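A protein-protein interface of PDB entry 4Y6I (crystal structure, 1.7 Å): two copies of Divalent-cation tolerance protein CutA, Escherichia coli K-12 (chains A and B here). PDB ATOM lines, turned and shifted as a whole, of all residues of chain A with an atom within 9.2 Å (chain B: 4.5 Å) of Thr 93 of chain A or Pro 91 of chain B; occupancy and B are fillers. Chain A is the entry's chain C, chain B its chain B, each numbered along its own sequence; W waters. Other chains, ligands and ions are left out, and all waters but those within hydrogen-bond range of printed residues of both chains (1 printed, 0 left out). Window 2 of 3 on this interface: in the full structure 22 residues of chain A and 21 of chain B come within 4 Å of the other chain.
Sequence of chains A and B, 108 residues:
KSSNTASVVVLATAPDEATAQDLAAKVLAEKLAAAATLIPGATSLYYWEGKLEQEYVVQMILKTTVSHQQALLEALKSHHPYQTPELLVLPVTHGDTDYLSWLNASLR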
ATOM      1  N   ALA A   6      -9.521 -25.810   3.331  1.00  0.00           N
ATOM      2  CA  ALA A   6      -9.531 -26.322   1.924  1.00  0.00           C
ATOM      3  C   ALA A   6     -10.544 -27.457   1.816  1.00  0.00           C
ATOM      4  O   ALA A   6     -10.984 -27.991   2.844  1.00  0.00           O
ATOM      5  CB  ALA A   6      -8.146 -26.792   1.518  1.00  0.00           C
ATOM      6  N   SER A   7     -10.892 -27.834   0.584  1.00  0.00           N
ATOM      7  CA  SER A   7     -11.926 -28.840   0.344  1.00  0.00           C
ATOM      8  C   SER A   7     -11.368 -30.135  -0.246  1.00  0.00           C
ATOM      9  O   SER A   7     -10.265 -30.153  -0.795  1.00  0.00           O
ATOM     10  CB  SER A   7     -13.013 -28.269  -0.567  1.00  0.00           C
ATOM     11  OG  SER A   7     -13.568 -27.085  -0.014  1.00  0.00           O
ATOM     12  N   VAL A   8     -12.131 -31.219  -0.105  1.00  0.00           N
ATOM     13  CA  VAL A   8     -11.761 -32.508  -0.684  1.00  0.00           C
ATOM     14  C   VAL A   8     -13.005 -33.179  -1.222  1.00  0.00           C
ATOM     15  O   VAL A   8     -14.134 -32.817  -0.861  1.00  0.00           O
ATOM     16  CB  VAL A   8     -11.126 -33.488   0.356  1.00  0.00           C
ATOM     17  CG1 VAL A   8      -9.794 -32.938   0.902  1.00  0.00           C
ATOM     18  CG2 VAL A   8     -12.112 -33.828   1.485  1.00  0.00           C
ATOM     19  N   VAL A   9     -12.791 -34.138  -2.110  1.00  0.00           N
ATOM     20  CA  VAL A   9     -13.876 -35.050  -2.471  1.00  0.00           C
ATOM     21  C   VAL A   9     -13.533 -36.438  -1.991  1.00  0.00           C
ATOM     22  O   VAL A   9     -12.362 -36.831  -1.926  1.00  0.00           O
ATOM     23  CB  VAL A   9     -14.260 -35.050  -3.975  1.00  0.00           C
ATOM     24  CG1 VAL A   9     -14.853 -33.693  -4.354  1.00  0.00           C
ATOM     25  CG2 VAL A   9     -13.066 -35.429  -4.861  1.00  0.00           C
ATOM     26  N   VAL A  89      -9.840 -40.267  -0.687  1.00  0.00           N
ATOM     27  CA  VAL A  89      -9.936 -38.806  -0.671  1.00  0.00           C
ATOM     28  C   VAL A  89      -9.053 -38.217  -1.774  1.00  0.00           C
ATOM     29  O   VAL A  89      -7.887 -38.587  -1.905  1.00  0.00           O
ATOM     30  CB  VAL A  89      -9.489 -38.239   0.689  1.00  0.00           C
ATOM     31  CG1 VAL A  89      -9.728 -36.735   0.751  1.00  0.00           C
ATOM     32  CG2 VAL A  89     -10.217 -38.963   1.831  1.00  0.00           C
ATOM     33  N   LEU A  90      -9.633 -37.307  -2.558  1.00  0.00           N
ATOM     34  CA  LEU A  90      -8.900 -36.559  -3.575  1.00  0.00           C
ATOM     35  C   LEU A  90      -8.928 -35.078  -3.207  1.00  0.00           C
ATOM     36  O   LEU A  90      -9.952 -34.569  -2.718  1.00  0.00           O
ATOM     37  CB  LEU A  90      -9.519 -36.762  -4.968  1.00  0.00           C
ATOM     38  CG  LEU A  90      -9.872 -38.182  -5.412  1.00  0.00           C
ATOM     39  CD1 LEU A  90     -10.549 -38.171  -6.772  1.00  0.00           C
ATOM     40  CD2 LEU A  90      -8.624 -39.047  -5.435  1.00  0.00           C
ATOM     41  N   PRO A  91      -7.804 -34.372  -3.425  1.00  0.00           N
ATOM     42  CA  PRO A  91      -7.779 -32.957  -3.076  1.00  0.00           C
ATOM     43  C   PRO A  91      -8.485 -32.088  -4.118  1.00  0.00           C
ATOM     44  O   PRO A  91      -8.426 -32.372  -5.315  1.00  0.00           O
ATOM     45  CB  PRO A  91      -6.285 -32.630  -3.046  1.00  0.00           C
ATOM     46  CG  PRO A  91      -5.657 -33.598  -3.988  1.00  0.00           C
ATOM     47  CD  PRO A  91      -6.510 -34.849  -3.960  1.00  0.00           C
ATOM     48  N   VAL A  92      -9.153 -31.054  -3.632  1.00  0.00           N
ATOM     49  CA  VAL A  92      -9.744 -30.020  -4.477  1.00  0.00           C
ATOM     50  C   VAL A  92      -8.865 -28.781  -4.327  1.00  0.00           C
ATOM     51  O   VAL A  92      -8.738 -28.245  -3.224  1.00  0.00           O
ATOM     52  CB  VAL A  92     -11.175 -29.696  -4.040  1.00  0.00           C
ATOM     53  CG1 VAL A  92     -11.724 -28.506  -4.826  1.00  0.00           C
ATOM     54  CG2 VAL A  92     -12.078 -30.894  -4.229  1.00  0.00           C
ATOM     55  N   THR A  93      -8.245 -28.351  -5.419  1.00  0.00           N
ATOM     56  CA  THR A  93      -7.324 -27.208  -5.371  1.00  0.00           C
ATOM     57  C   THR A  93      -8.063 -25.868  -5.382  1.00  0.00           C
ATOM     58  O   THR A  93      -7.653 -24.913  -4.702  1.00  0.00           O
ATOM     59  CB  THR A  93      -6.278 -27.244  -6.540  1.00  0.00           C
ATOM     60  OG1 THR A  93      -6.927 -26.986  -7.784  1.00  0.00           O
ATOM     61  CG2 THR A  93      -5.555 -28.580  -6.616  1.00  0.00           C
ATOM     62  N   HIS A  94      -9.143 -25.806  -6.171  1.00  0.00           N
ATOM     63  CA  HIS A  94      -9.901 -24.582  -6.437  1.00  0.00           C
ATOM     64  C   HIS A  94     -11.325 -24.959  -6.762  1.00  0.00           C
ATOM     65  O   HIS A  94     -11.609 -26.111  -7.061  1.00  0.00           O
ATOM     66  CB  HIS A  94      -9.299 -23.829  -7.624  1.00  0.00           C
ATOM     67  CG  HIS A  94      -7.899 -23.365  -7.376  1.00  0.00           C
ATOM     68  ND1 HIS A  94      -6.799 -24.166  -7.593  1.00  0.00           N
ATOM     69  CD2 HIS A  94      -7.423 -22.190  -6.900  1.00  0.00           C
ATOM     70  CE1 HIS A  94      -5.704 -23.505  -7.256  1.00  0.00           C
ATOM     71  NE2 HIS A  94      -6.058 -22.303  -6.833  1.00  0.00           N
ATOM     72  N   GLY A  95     -12.230 -23.988  -6.731  1.00  0.00           N
ATOM     73  CA  GLY A  95     -13.609 -24.268  -7.112  1.00  0.00           C
ATOM     74  C   GLY A  95     -14.427 -23.001  -7.124  1.00  0.00           C
ATOM     75  O   GLY A  95     -13.887 -21.925  -6.867  1.00  0.00           O
ATOM     76  N   ASP A  96     -15.719 -23.123  -7.415  1.00  0.00           N
ATOM     77  CA  ASP A  96     -16.606 -21.964  -7.418  1.00  0.00           C
ATOM     78  C   ASP A  96     -16.562 -21.331  -6.021  1.00  0.00           C
ATOM     79  O   ASP A  96     -16.778 -22.016  -5.031  1.00  0.00           O
ATOM     80  CB  ASP A  96     -18.023 -22.377  -7.792  1.00  0.00           C
ATOM     81  CG  ASP A  96     -18.982 -21.211  -7.788  1.00  0.00           C
ATOM     82  OD1 ASP A  96     -19.135 -20.582  -8.854  1.00  0.00           O
ATOM     83  OD2 ASP A  96     -19.551 -20.914  -6.716  1.00  0.00           O
ATOM     84  N   LEU A 100     -17.747 -23.099  -2.535  1.00  0.00           N
ATOM     85  CA  LEU A 100     -16.802 -23.443  -1.459  1.00  0.00           C
ATOM     86  C   LEU A 100     -17.183 -22.769  -0.142  1.00  0.00           C
ATOM     87  O   LEU A 100     -17.029 -23.358   0.932  1.00  0.00           O
ATOM     88  CB  LEU A 100     -15.354 -23.130  -1.851  1.00  0.00           C
ATOM     89  CG  LEU A 100     -14.774 -23.943  -3.018  1.00  0.00           C
ATOM     90  CD1 LEU A 100     -13.413 -23.405  -3.411  1.00  0.00           C
ATOM     91  CD2 LEU A 100     -14.717 -25.452  -2.702  1.00  0.00           C
ATOM     92  N   GLN B  69      -8.078 -22.811 -15.934  1.00  0.00           N
ATOM     93  CA  GLN B  69      -9.078 -23.290 -14.984  1.00  0.00           C
ATOM     94  C   GLN B  69      -9.973 -22.191 -14.455  1.00  0.00           C
ATOM     95  O   GLN B  69     -11.167 -22.407 -14.306  1.00  0.00           O
ATOM     96  CB  GLN B  69      -8.452 -24.098 -13.842  1.00  0.00           C
ATOM     97  CG  GLN B  69      -7.585 -23.310 -12.891  1.00  0.00           C
ATOM     98  CD  GLN B  69      -7.017 -24.164 -11.785  1.00  0.00           C
ATOM     99  OE1 GLN B  69      -6.426 -25.211 -12.029  1.00  0.00           O
ATOM    100  NE2 GLN B  69      -7.205 -23.723 -10.548  1.00  0.00           N
ATOM    101  N   VAL B  89     -12.076 -28.164  -8.845  1.00  0.00           N
ATOM    102  CA  VAL B  89     -10.864 -28.474  -9.627  1.00  0.00           C
ATOM    103  C   VAL B  89      -9.995 -29.493  -8.883  1.00  0.00           C
ATOM    104  O   VAL B  89      -9.659 -29.277  -7.718  1.00  0.00           O
ATOM    105  CB  VAL B  89     -10.017 -27.216  -9.879  1.00  0.00           C
ATOM    106  CG1 VAL B  89      -8.778 -27.553 -10.770  1.00  0.00           C
ATOM    107  CG2 VAL B  89     -10.866 -26.143 -10.526  1.00  0.00           C
ATOM    108  N   LEU B  90      -9.643 -30.579  -9.580  1.00  0.00           N
ATOM    109  CA  LEU B  90      -8.770 -31.631  -9.043  1.00  0.00           C
ATOM    110  C   LEU B  90      -7.462 -31.649  -9.829  1.00  0.00           C
ATOM    111  O   LEU B  90      -7.476 -31.476 -11.054  1.00  0.00           O
ATOM    112  CB  LEU B  90      -9.440 -33.008  -9.156  1.00  0.00           C
ATOM    113  CG  LEU B  90     -10.899 -33.182  -8.730  1.00  0.00           C
ATOM    114  CD1 LEU B  90     -11.339 -34.622  -8.950  1.00  0.00           C
ATOM    115  CD2 LEU B  90     -11.096 -32.788  -7.279  1.00  0.00           C
ATOM    116  N   PRO B  91      -6.325 -31.877  -9.144  1.00  0.00           N
ATOM    117  CA  PRO B  91      -5.054 -31.875  -9.879  1.00  0.00           C
ATOM    118  C   PRO B  91      -4.800 -33.183 -10.620  1.00  0.00           C
ATOM    119  O   PRO B  91      -5.195 -34.243 -10.147  1.00  0.00           O
ATOM    120  CB  PRO B  91      -4.011 -31.713  -8.767  1.00  0.00           C
ATOM    121  CG  PRO B  91      -4.648 -32.366  -7.566  1.00  0.00           C
ATOM    122  CD  PRO B  91      -6.139 -32.159  -7.706  1.00  0.00           C
ATOM    123  N   VAL B  92      -4.167 -33.092 -11.786  1.00  0.00           N
ATOM    124  CA  VAL B  92      -3.718 -34.270 -12.523  1.00  0.00           C
ATOM    125  C   VAL B  92      -2.207 -34.334 -12.352  1.00  0.00           C
ATOM    126  O   VAL B  92      -1.481 -33.438 -12.806  1.00  0.00           O
ATOM    127  CB  VAL B  92      -4.076 -34.166 -14.009  1.00  0.00           C
ATOM    128  CG1 VAL B  92      -3.454 -35.295 -14.803  1.00  0.00           C
ATOM    129  CG2 VAL B  92      -5.591 -34.143 -14.201  1.00  0.00           C
ATOM    130  N   THR B  93      -1.742 -35.376 -11.676  1.00  0.00           N
ATOM    131  CA  THR B  93      -0.321 -35.477 -11.324  1.00  0.00           C
ATOM    132  C   THR B  93       0.505 -36.193 -12.379  1.00  0.00           C
ATOM    133  O   THR B  93       1.741 -36.054 -12.412  1.00  0.00           O
ATOM    134  CB  THR B  93      -0.136 -36.154  -9.959  1.00  0.00           C
ATOM    135  OG1 THR B  93      -0.978 -37.318  -9.880  1.00  0.00           O
ATOM    136  CG2 THR B  93      -0.503 -35.184  -8.843  1.00  0.00           C
HETATM  137  O   HOH W   1      -5.245 -26.479  -9.979  1.00  0.00           O
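Of the 13 printed residues of chain A, 4 touch a printed residue of chain B. Hydrophobic or aromatic side chains of chain A within 4 Å of the printed part of chain B: Pro 91, Val 92 and His 94. Among the printed residues, 8 pairs touch across the chains. Among the printed residues, no Asp or Glu carboxylate lies within 4 Å of a Lys or Arg side-chain nitrogen of the other chain.
Pro 91 of chain A touches Leu 90 of chain B. O of Pro 91 of chain A touches CD of Pro 91 of chain B, 3.3 Å away. Val 92 of chain A touches Val 89 of chain B (CA to O, 3.3 Å). Leu 90 of chain B touches Val 92 of chain A (CD2 to CG2, 3.7 Å). CG2 of Thr 93 of chain A touches CD of Pro 91 of chain B, 3.8 Å away.
Pro 91 of chain A touches Leu 90 of chain B, but with the chains exchanged Leu 90 of chain A does not touch Pro 91 of chain B (6.0 Å). Val 92 of chain A touches Val 89 of chain B, but with the chains exchanged Val 89 of chain A does not touch Val 92 of chain B (11.9 Å). Val 92 of chain A touches Leu 90 of chain B, but with the chains exchanged Leu 90 of chain A does not touch Val 92 of chain B (9.4 Å). Thr 93 of chain A touches Pro 91 of chain B, but with the chains exchanged Pro 91 of chain A does not touch Thr 93 of chain B (7.3 Å). Positions printed for both chains: 89, 90, 91, 92 and 93.
ND1 of His 94 of chain A sits at hydrogen-bond distance from NE2 of Gln 69 of chain B (3.0 Å). N of Thr 93 of chain A is in hydrogen-bond range of O of Val 89 of chain B (2.9 Å). The backbone carbonyl oxygen of His 94 of chain A sits at hydrogen-bond distance from the backbone NH of Val 89 of chain B, at 2.8 Å.
Of the printed residues of chain B, Thr 93 of chain A touches Val 89 and Pro 91. Of chain A, only Pro 91 and Thr 93 come within 4 Å of Pro 91 of chain B. Of chain A, only Val 92 (3.3 Å), Thr 93 (2.9 Å) and His 94 (2.8 Å) come within 4 Å of Val 89 of chain B. No residue of chain A comes within 4 Å of Val 92 of chain B. Printed residues of chain B within 4 Å of Val 92 of chain A: Val 89 (3.3 Å) and Leu 90 (3.7 Å). Of the printed residues of chain B, Pro 91 of chain A touches Leu 90 (3.3 Å) and Pro 91 (3.3 Å). Of the printed residues of chain A, Gln 69 of chain B touches His 94 (3.0 Å). Printed residues of chain B within 4 Å of His 94 of chain A: Gln 69 and Val 89. Of the printed residues of chain A, Leu 90 of chain B touches Pro 91 (3.3 Å) and Val 92 (3.7 Å). Thr 93 of chain B touches none of the printed residues of chain A. Val 8 of chain A touches none of the printed residues of chain B. The nearest residue of chain B that does not touch Thr 93 of chain A is Gln 69 of chain B (4.3 Å). The nearest printed residue of chain B that does not touch Val 92 of chain A is Pro 91 of chain B (5.2 Å).
O of Ser 7 of chain A is in hydrogen-bond range of N of Val 92 of chain A, 3.2 Å away. A ring nitrogen (ND1) of His 94 of chain A lies within hydrogen-bond range of the side-chain hydroxyl (OG1) of Thr 93 of chain A.
Water W1 lies within hydrogen-bond range of the side-chain amide oxygen (OE1) of Gln 69 of chain B (2.7 Å) and the side-chain hydroxyl (OG1) of Thr 93 of chain A (2.8 Å).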
